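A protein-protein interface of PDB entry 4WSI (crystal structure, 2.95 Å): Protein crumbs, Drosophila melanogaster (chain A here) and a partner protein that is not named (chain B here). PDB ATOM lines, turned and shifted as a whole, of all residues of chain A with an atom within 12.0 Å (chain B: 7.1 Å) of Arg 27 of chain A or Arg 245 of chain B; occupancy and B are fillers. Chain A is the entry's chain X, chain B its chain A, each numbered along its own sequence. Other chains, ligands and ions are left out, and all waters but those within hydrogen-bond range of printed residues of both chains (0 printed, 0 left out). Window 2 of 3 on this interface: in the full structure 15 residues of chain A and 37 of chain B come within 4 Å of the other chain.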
ATOM      1  N   PRO A  26     -22.402 -14.821  -4.840  1.00  0.00           N
ATOM      2  CA  PRO A  26     -21.042 -14.415  -5.206  1.00  0.00           C
ATOM      3  C   PRO A  26     -20.599 -13.177  -4.439  1.00  0.00           C
ATOM      4  O   PRO A  26     -21.437 -12.450  -3.906  1.00  0.00           O
ATOM      5  CB  PRO A  26     -21.180 -14.070  -6.688  1.00  0.00           C
ATOM      6  CG  PRO A  26     -22.582 -13.595  -6.813  1.00  0.00           C
ATOM      7  CD  PRO A  26     -23.373 -14.490  -5.898  1.00  0.00           C
ATOM      8  N   ARG A  27     -19.291 -12.941  -4.392  1.00  0.00           N
ATOM      9  CA  ARG A  27     -18.749 -11.753  -3.745  1.00  0.00           C
ATOM     10  C   ARG A  27     -18.416 -10.703  -4.793  1.00  0.00           C
ATOM     11  O   ARG A  27     -17.476 -10.870  -5.568  1.00  0.00           O
ATOM     12  CB  ARG A  27     -17.496 -12.098  -2.943  1.00  0.00           C
ATOM     13  CG  ARG A  27     -17.738 -13.083  -1.818  1.00  0.00           C
ATOM     14  CD  ARG A  27     -16.442 -13.445  -1.116  1.00  0.00           C
ATOM     15  NE  ARG A  27     -16.658 -14.431  -0.062  1.00  0.00           N
ATOM     16  CZ  ARG A  27     -16.676 -15.743  -0.263  1.00  0.00           C
ATOM     17  NH1 ARG A  27     -16.490 -16.231  -1.483  1.00  0.00           N
ATOM     18  NH2 ARG A  27     -16.881 -16.568   0.755  1.00  0.00           N
ATOM     19  N   LEU A  28     -19.190  -9.622  -4.807  1.00  0.00           N
ATOM     20  CA  LEU A  28     -19.055  -8.590  -5.829  1.00  0.00           C
ATOM     21  C   LEU A  28     -17.654  -7.987  -5.844  1.00  0.00           C
ATOM     22  O   LEU A  28     -17.081  -7.746  -6.909  1.00  0.00           O
ATOM     23  CB  LEU A  28     -20.101  -7.494  -5.612  1.00  0.00           C
ATOM     24  CG  LEU A  28     -21.536  -7.979  -5.388  1.00  0.00           C
ATOM     25  CD1 LEU A  28     -22.478  -6.803  -5.175  1.00  0.00           C
ATOM     26  CD2 LEU A  28     -22.010  -8.851  -6.545  1.00  0.00           C
ATOM     27  N   GLU A  29     -17.101  -7.763  -4.657  1.00  0.00           N
ATOM     28  CA  GLU A  29     -15.791  -7.135  -4.518  1.00  0.00           C
ATOM     29  C   GLU A  29     -14.659  -7.962  -5.134  1.00  0.00           C
ATOM     30  O   GLU A  29     -13.750  -7.416  -5.760  1.00  0.00           O
ATOM     31  CB  GLU A  29     -15.497  -6.841  -3.042  1.00  0.00           C
ATOM     32  CG  GLU A  29     -16.411  -5.789  -2.416  1.00  0.00           C
ATOM     33  CD  GLU A  29     -17.646  -6.377  -1.754  1.00  0.00           C
ATOM     34  OE1 GLU A  29     -17.760  -7.618  -1.694  1.00  0.00           O
ATOM     35  OE2 GLU A  29     -18.501  -5.594  -1.288  1.00  0.00           O
ATOM     36  N   MET A  30     -14.726  -9.279  -4.961  1.00  0.00           N
ATOM     37  CA  MET A  30     -13.673 -10.177  -5.430  1.00  0.00           C
ATOM     38  C   MET A  30     -13.613 -10.275  -6.951  1.00  0.00           C
ATOM     39  O   MET A  30     -12.576 -10.618  -7.516  1.00  0.00           O
ATOM     40  CB  MET A  30     -13.845 -11.570  -4.822  1.00  0.00           C
ATOM     41  CG  MET A  30     -13.722 -11.604  -3.311  1.00  0.00           C
ATOM     42  SD  MET A  30     -12.094 -11.086  -2.744  1.00  0.00           S
ATOM     43  CE  MET A  30     -11.068 -12.357  -3.480  1.00  0.00           C
ATOM     44  N   ASP A  31     -14.730  -9.984  -7.609  1.00  0.00           N
ATOM     45  CA  ASP A  31     -14.771  -9.979  -9.067  1.00  0.00           C
ATOM     46  C   ASP A  31     -14.147  -8.701  -9.613  1.00  0.00           C
ATOM     47  O   ASP A  31     -13.634  -8.676 -10.731  1.00  0.00           O
ATOM     48  CB  ASP A  31     -16.206 -10.132  -9.572  1.00  0.00           C
ATOM     49  CG  ASP A  31     -16.684 -11.570  -9.541  1.00  0.00           C
ATOM     50  OD1 ASP A  31     -16.023 -12.409  -8.889  1.00  0.00           O
ATOM     51  OD2 ASP A  31     -17.722 -11.864 -10.169  1.00  0.00           O
ATOM     52  N   ASN A  32     -14.186  -7.644  -8.808  1.00  0.00           N
ATOM     53  CA  ASN A  32     -13.596  -6.366  -9.187  1.00  0.00           C
ATOM     54  C   ASN A  32     -12.074  -6.381  -9.158  1.00  0.00           C
ATOM     55  O   ASN A  32     -11.426  -5.891 -10.081  1.00  0.00           O
ATOM     56  CB  ASN A  32     -14.113  -5.246  -8.284  1.00  0.00           C
ATOM     57  CG  ASN A  32     -15.346  -4.577  -8.843  1.00  0.00           C
ATOM     58  OD1 ASN A  32     -15.250  -3.703  -9.705  1.00  0.00           O
ATOM     59  ND2 ASN A  32     -16.513  -4.980  -8.353  1.00  0.00           N
ATOM     60  N   VAL A  33     -11.508  -6.944  -8.095  1.00  0.00           N
ATOM     61  CA  VAL A  33     -10.057  -6.995  -7.941  1.00  0.00           C
ATOM     62  C   VAL A  33      -9.384  -7.874  -8.998  1.00  0.00           C
ATOM     63  O   VAL A  33      -8.166  -7.832  -9.163  1.00  0.00           O
ATOM     64  CB  VAL A  33      -9.649  -7.457  -6.524  1.00  0.00           C
ATOM     65  CG1 VAL A  33     -10.027  -6.406  -5.495  1.00  0.00           C
ATOM     66  CG2 VAL A  33     -10.291  -8.793  -6.186  1.00  0.00           C
ATOM     67  N   LEU A  34     -10.185  -8.661  -9.712  1.00  0.00           N
ATOM     68  CA  LEU A  34      -9.690  -9.489 -10.808  1.00  0.00           C
ATOM     69  C   LEU A  34      -9.366  -8.652 -12.039  1.00  0.00           C
ATOM     70  O   LEU A  34      -8.563  -9.052 -12.882  1.00  0.00           O
ATOM     71  CB  LEU A  34     -10.724 -10.548 -11.182  1.00  0.00           C
ATOM     72  CG  LEU A  34     -10.755 -11.802 -10.315  1.00  0.00           C
ATOM     73  CD1 LEU A  34     -11.941 -12.670 -10.694  1.00  0.00           C
ATOM     74  CD2 LEU A  34      -9.453 -12.567 -10.471  1.00  0.00           C
ATOM     75  N   LYS A  35     -10.012  -7.496 -12.142  1.00  0.00           N
ATOM     76  CA  LYS A  35      -9.774  -6.579 -13.247  1.00  0.00           C
ATOM     77  C   LYS A  35      -8.375  -5.986 -13.134  1.00  0.00           C
ATOM     78  O   LYS A  35      -7.860  -5.824 -12.027  1.00  0.00           O
ATOM     79  CB  LYS A  35     -10.841  -5.480 -13.257  1.00  0.00           C
ATOM     80  CG  LYS A  35     -12.202  -5.971 -13.732  1.00  0.00           C
ATOM     81  CD  LYS A  35     -13.332  -5.475 -12.846  1.00  0.00           C
ATOM     82  CE  LYS A  35     -14.648  -6.143 -13.228  1.00  0.00           C
ATOM     83  NZ  LYS A  35     -15.785  -5.709 -12.367  1.00  0.00           N
ATOM     84  N   ARG B 215     -17.422 -20.250 -13.391  1.00  0.00           N
ATOM     85  CA  ARG B 215     -17.253 -20.483 -11.960  1.00  0.00           C
ATOM     86  C   ARG B 215     -18.595 -20.653 -11.266  1.00  0.00           C
ATOM     87  O   ARG B 215     -18.855 -21.681 -10.642  1.00  0.00           O
ATOM     88  CB  ARG B 215     -16.497 -19.327 -11.305  1.00  0.00           C
ATOM     89  CG  ARG B 215     -15.022 -19.584 -11.096  1.00  0.00           C
ATOM     90  CD  ARG B 215     -14.473 -18.756  -9.946  1.00  0.00           C
ATOM     91  NE  ARG B 215     -14.545 -17.320 -10.196  1.00  0.00           N
ATOM     92  CZ  ARG B 215     -15.460 -16.513  -9.670  1.00  0.00           C
ATOM     93  NH1 ARG B 215     -15.444 -15.217  -9.955  1.00  0.00           N
ATOM     94  NH2 ARG B 215     -16.389 -17.001  -8.858  1.00  0.00           N
ATOM     95  N   GLN B 216     -19.442 -19.634 -11.378  1.00  0.00           N
ATOM     96  CA  GLN B 216     -20.744 -19.637 -10.722  1.00  0.00           C
ATOM     97  C   GLN B 216     -21.615 -20.786 -11.215  1.00  0.00           C
ATOM     98  O   GLN B 216     -22.405 -21.343 -10.453  1.00  0.00           O
ATOM     99  CB  GLN B 216     -21.454 -18.296 -10.919  1.00  0.00           C
ATOM    100  CG  GLN B 216     -20.751 -17.129 -10.246  1.00  0.00           C
ATOM    101  CD  GLN B 216     -20.555 -17.354  -8.760  1.00  0.00           C
ATOM    102  OE1 GLN B 216     -19.437 -17.591  -8.298  1.00  0.00           O
ATOM    103  NE2 GLN B 216     -21.643 -17.283  -8.001  1.00  0.00           N
ATOM    104  N   MET B 219     -20.231 -23.601  -9.172  1.00  0.00           N
ATOM    105  CA  MET B 219     -20.574 -23.422  -7.764  1.00  0.00           C
ATOM    106  C   MET B 219     -22.042 -23.719  -7.469  1.00  0.00           C
ATOM    107  O   MET B 219     -22.381 -24.138  -6.364  1.00  0.00           O
ATOM    108  CB  MET B 219     -20.241 -21.996  -7.318  1.00  0.00           C
ATOM    109  CG  MET B 219     -18.755 -21.681  -7.267  1.00  0.00           C
ATOM    110  SD  MET B 219     -17.971 -22.198  -5.727  1.00  0.00           S
ATOM    111  CE  MET B 219     -18.806 -21.139  -4.548  1.00  0.00           C
ATOM    112  N   SER B 228     -15.425 -22.079  -2.051  1.00  0.00           N
ATOM    113  CA  SER B 228     -14.572 -20.930  -2.314  1.00  0.00           C
ATOM    114  C   SER B 228     -13.777 -20.565  -1.071  1.00  0.00           C
ATOM    115  O   SER B 228     -14.310 -20.563   0.037  1.00  0.00           O
ATOM    116  CB  SER B 228     -15.405 -19.732  -2.772  1.00  0.00           C
ATOM    117  OG  SER B 228     -16.149 -19.187  -1.696  1.00  0.00           O
ATOM    118  N   ALA B 229     -12.497 -20.269  -1.260  1.00  0.00           N
ATOM    119  CA  ALA B 229     -11.657 -19.818  -0.164  1.00  0.00           C
ATOM    120  C   ALA B 229     -12.214 -18.513   0.391  1.00  0.00           C
ATOM    121  O   ALA B 229     -12.572 -17.613  -0.366  1.00  0.00           O
ATOM    122  CB  ALA B 229     -10.222 -19.628  -0.636  1.00  0.00           C
ATOM    123  N   VAL B 230     -12.307 -18.425   1.713  1.00  0.00           N
ATOM    124  CA  VAL B 230     -12.811 -17.220   2.358  1.00  0.00           C
ATOM    125  C   VAL B 230     -11.744 -16.135   2.321  1.00  0.00           C
ATOM    126  O   VAL B 230     -10.712 -16.249   2.986  1.00  0.00           O
ATOM    127  CB  VAL B 230     -13.240 -17.489   3.816  1.00  0.00           C
ATOM    128  CG1 VAL B 230     -13.701 -16.200   4.476  1.00  0.00           C
ATOM    129  CG2 VAL B 230     -14.341 -18.532   3.857  1.00  0.00           C
ATOM    130  N   PRO B 231     -11.987 -15.080   1.533  1.00  0.00           N
ATOM    131  CA  PRO B 231     -10.985 -14.026   1.363  1.00  0.00           C
ATOM    132  C   PRO B 231     -10.933 -13.106   2.570  1.00  0.00           C
ATOM    133  O   PRO B 231     -11.788 -13.186   3.447  1.00  0.00           O
ATOM    134  CB  PRO B 231     -11.491 -13.264   0.137  1.00  0.00           C
ATOM    135  CG  PRO B 231     -12.955 -13.459   0.161  1.00  0.00           C
ATOM    136  CD  PRO B 231     -13.214 -14.810   0.764  1.00  0.00           C
ATOM    137  N   GLN B 240     -25.854  -8.336   7.588  1.00  0.00           N
ATOM    138  CA  GLN B 240     -26.122  -9.736   7.277  1.00  0.00           C
ATOM    139  C   GLN B 240     -24.882 -10.428   6.726  1.00  0.00           C
ATOM    140  O   GLN B 240     -24.959 -11.199   5.771  1.00  0.00           O
ATOM    141  CB  GLN B 240     -27.291  -9.861   6.294  1.00  0.00           C
ATOM    142  CG  GLN B 240     -28.632  -9.436   6.874  1.00  0.00           C
ATOM    143  CD  GLN B 240     -29.803 -10.075   6.155  1.00  0.00           C
ATOM    144  OE1 GLN B 240     -29.641 -11.063   5.438  1.00  0.00           O
ATOM    145  NE2 GLN B 240     -30.991  -9.514   6.342  1.00  0.00           N
ATOM    146  N   GLU B 241     -23.737 -10.136   7.331  1.00  0.00           N
ATOM    147  CA  GLU B 241     -22.501 -10.828   6.998  1.00  0.00           C
ATOM    148  C   GLU B 241     -21.917 -11.511   8.225  1.00  0.00           C
ATOM    149  O   GLU B 241     -22.032 -11.008   9.344  1.00  0.00           O
ATOM    150  CB  GLU B 241     -21.479  -9.872   6.388  1.00  0.00           C
ATOM    151  CG  GLU B 241     -21.805  -9.457   4.966  1.00  0.00           C
ATOM    152  CD  GLU B 241     -20.715  -8.617   4.340  1.00  0.00           C
ATOM    153  OE1 GLU B 241     -20.023  -7.885   5.079  1.00  0.00           O
ATOM    154  OE2 GLU B 241     -20.547  -8.689   3.105  1.00  0.00           O
ATOM    155  N   VAL B 242     -21.295 -12.663   8.004  1.00  0.00           N
ATOM    156  CA  VAL B 242     -20.714 -13.441   9.088  1.00  0.00           C
ATOM    157  C   VAL B 242     -19.192 -13.392   9.020  1.00  0.00           C
ATOM    158  O   VAL B 242     -18.606 -13.549   7.949  1.00  0.00           O
ATOM    159  CB  VAL B 242     -21.172 -14.905   9.029  1.00  0.00           C
ATOM    160  CG1 VAL B 242     -20.791 -15.628  10.311  1.00  0.00           C
ATOM    161  CG2 VAL B 242     -22.674 -14.980   8.797  1.00  0.00           C
ATOM    162  N   ALA B 243     -18.557 -13.191  10.171  1.00  0.00           N
ATOM    163  CA  ALA B 243     -17.110 -13.003  10.239  1.00  0.00           C
ATOM    164  C   ALA B 243     -16.314 -14.258   9.887  1.00  0.00           C
ATOM    165  O   ALA B 243     -15.086 -14.225   9.836  1.00  0.00           O
ATOM    166  CB  ALA B 243     -16.707 -12.491  11.614  1.00  0.00           C
ATOM    167  N   GLY B 244     -17.010 -15.359   9.642  1.00  0.00           N
ATOM    168  CA  GLY B 244     -16.344 -16.611   9.348  1.00  0.00           C
ATOM    169  C   GLY B 244     -16.367 -17.001   7.885  1.00  0.00           C
ATOM    170  O   GLY B 244     -15.339 -17.372   7.323  1.00  0.00           O
ATOM    171  N   ARG B 245     -17.540 -16.918   7.263  1.00  0.00           N
ATOM    172  CA  ARG B 245     -17.718 -17.447   5.915  1.00  0.00           C
ATOM    173  C   ARG B 245     -17.678 -16.394   4.809  1.00  0.00           C
ATOM    174  O   ARG B 245     -17.138 -16.648   3.733  1.00  0.00           O
ATOM    175  CB  ARG B 245     -19.004 -18.277   5.815  1.00  0.00           C
ATOM    176  CG  ARG B 245     -20.270 -17.544   6.217  1.00  0.00           C
ATOM    177  CD  ARG B 245     -21.501 -18.265   5.694  1.00  0.00           C
ATOM    178  NE  ARG B 245     -22.738 -17.665   6.188  1.00  0.00           N
ATOM    179  CZ  ARG B 245     -23.359 -16.640   5.611  1.00  0.00           C
ATOM    180  NH1 ARG B 245     -22.857 -16.091   4.513  1.00  0.00           N
ATOM    181  NH2 ARG B 245     -24.479 -16.163   6.134  1.00  0.00           N
ATOM    182  N   ASP B 246     -18.253 -15.225   5.061  1.00  0.00           N
ATOM    183  CA  ASP B 246     -18.278 -14.181   4.043  1.00  0.00           C
ATOM    184  C   ASP B 246     -16.881 -13.637   3.774  1.00  0.00           C
ATOM    185  O   ASP B 246     -16.384 -13.699   2.651  1.00  0.00           O
ATOM    186  CB  ASP B 246     -19.235 -13.060   4.446  1.00  0.00           C
ATOM    187  CG  ASP B 246     -20.683 -13.474   4.334  1.00  0.00           C
ATOM    188  OD1 ASP B 246     -21.064 -14.000   3.268  1.00  0.00           O
ATOM    189  OD2 ASP B 246     -21.433 -13.292   5.313  1.00  0.00           O
ATOM    190  N   TYR B 247     -16.252 -13.112   4.818  1.00  0.00           N
ATOM    191  CA  TYR B 247     -14.883 -12.632   4.735  1.00  0.00           C
ATOM    192  C   TYR B 247     -14.215 -12.826   6.081  1.00  0.00           C
ATOM    193  O   TYR B 247     -14.890 -12.951   7.101  1.00  0.00           O
ATOM    194  CB  TYR B 247     -14.850 -11.140   4.397  1.00  0.00           C
ATOM    195  CG  TYR B 247     -15.135 -10.791   2.957  1.00  0.00           C
ATOM    196  CD1 TYR B 247     -14.112 -10.730   2.023  1.00  0.00           C
ATOM    197  CD2 TYR B 247     -16.423 -10.495   2.533  1.00  0.00           C
ATOM    198  CE1 TYR B 247     -14.364 -10.401   0.707  1.00  0.00           C
ATOM    199  CE2 TYR B 247     -16.684 -10.167   1.219  1.00  0.00           C
ATOM    200  CZ  TYR B 247     -15.651 -10.122   0.310  1.00  0.00           C
ATOM    201  OH  TYR B 247     -15.902  -9.796  -1.003  1.00  0.00           O
ATOM    202  N   HIS B 248     -12.890 -12.852   6.084  1.00  0.00           N
ATOM    203  CA  HIS B 248     -12.153 -12.681   7.322  1.00  0.00           C
ATOM    204  C   HIS B 248     -11.948 -11.186   7.515  1.00  0.00           C
ATOM    205  O   HIS B 248     -11.015 -10.607   6.959  1.00  0.00           O
ATOM    206  CB  HIS B 248     -10.813 -13.406   7.265  1.00  0.00           C
ATOM    207  CG  HIS B 248     -10.927 -14.894   7.393  1.00  0.00           C
ATOM    208  ND1 HIS B 248     -10.894 -15.741   6.307  1.00  0.00           N
ATOM    209  CD2 HIS B 248     -11.088 -15.682   8.481  1.00  0.00           C
ATOM    210  CE1 HIS B 248     -11.022 -16.988   6.720  1.00  0.00           C
ATOM    211  NE2 HIS B 248     -11.141 -16.981   8.035  1.00  0.00           N
ATOM    212  N   PHE B 249     -12.835 -10.558   8.284  1.00  0.00           N
ATOM    213  CA  PHE B 249     -12.802  -9.109   8.452  1.00  0.00           C
ATOM    214  C   PHE B 249     -11.694  -8.686   9.403  1.00  0.00           C
ATOM    215  O   PHE B 249     -11.740  -8.978  10.598  1.00  0.00           O
ATOM    216  CB  PHE B 249     -14.158  -8.585   8.927  1.00  0.00           C
ATOM    217  CG  PHE B 249     -15.300  -8.929   8.006  1.00  0.00           C
ATOM    218  CD1 PHE B 249     -15.681  -8.064   6.995  1.00  0.00           C
ATOM    219  CD2 PHE B 249     -15.991 -10.121   8.152  1.00  0.00           C
ATOM    220  CE1 PHE B 249     -16.728  -8.382   6.145  1.00  0.00           C
ATOM    221  CE2 PHE B 249     -17.040 -10.442   7.311  1.00  0.00           C
ATOM    222  CZ  PHE B 249     -17.409  -9.573   6.306  1.00  0.00           C
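The guanidinium group (NE) of Arg 27 of chain A sits at hydrogen-bond distance from the backbone carbonyl oxygen (O) of Asp 246 of chain B. The side-chain hydroxyl (OH) of Tyr 247 of chain B sits at hydrogen-bond distance from the side-chain carboxylate (OE1) of Glu 29 of chain A, 2.9 Å away. NH1 of Arg 215 of chain B is in salt-bridge range of OD1 of Asp 31 of chain A (3.1 Å). OG of Ser 228 of chain B is in hydrogen-bond range of NH1 of Arg 27 of chain A (3.0 Å). The backbone carbonyl oxygen (O) of Arg 245 of chain B lies within hydrogen-bond range of the guanidinium group (NH2) of Arg 27 of chain A (3.0 Å).
NH1 of Arg 245 of chain B is in salt-bridge range of OD1 of Asp 246 of chain B (3.0 Å). The side-chain amide oxygen (OE1) of Gln 216 of chain B sits at hydrogen-bond distance from the guanidinium group (NH2) of Arg 215 of chain B, 3.2 Å away. The backbone carbonyl oxygen (O) of Pro 231 of chain B sits at hydrogen-bond distance from the backbone NH (N) of His 248 of chain B, at 2.9 Å. The side-chain carboxylate (OD2) of Asp 246 of chain B is in hydrogen-bond range of the backbone NH (N) of Val 242 of chain B (2.8 Å).
NE2 of Gln 216 of chain B touches CB of Pro 26 of chain A, at 3.5 Å. CD of Pro 231 of chain B touches NE of Arg 27 of chain A, 3.6 Å away. Tyr 247 of chain B touches Arg 27 of chain A (OH to CB, 3.4 Å). Pro 231 of chain B touches Met 30 of chain A (CB to SD, 3.7 Å). Tyr 247 of chain B touches Met 30 of chain A.
Arg 27 of chain A touches just these residues of chain B: Ser 228, Pro 231, Arg 245, Asp 246 and Tyr 247. Of the printed residues of chain B, Glu 29 of chain A touches Tyr 247. Printed residues of chain A within 4 Å of Gln 216 of chain B: Pro 26. No residue of chain A comes within 4 Å of Ala 229 of chain B. No residue of chain A comes within 4 Å of Val 230 of chain B. No residue of chain A comes within 4 Å of Val 242 of chain B. Of chain A, only Arg 27 (3.0 Å) comes within 4 Å of Arg 245 of chain B. Of chain A, only Arg 27 (2.8 Å) comes within 4 Å of Asp 246 of chain B. Tyr 247 of chain B touches just these residues of chain A: Arg 27 (3.4 Å), Glu 29 (2.9 Å) and Met 30 (3.7 Å). The nearest residue of chain A that does not touch Arg 245 of chain B is Pro 26 of chain A (9.3 Å).
Hydrophobic or aromatic side chains of chain B within 4 Å of the printed part of chain A: Pro 231 and Tyr 247. Hydrophobic or aromatic side chains of chain A within 4 Å of the printed part of chain B: Pro 26 and Met 30.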
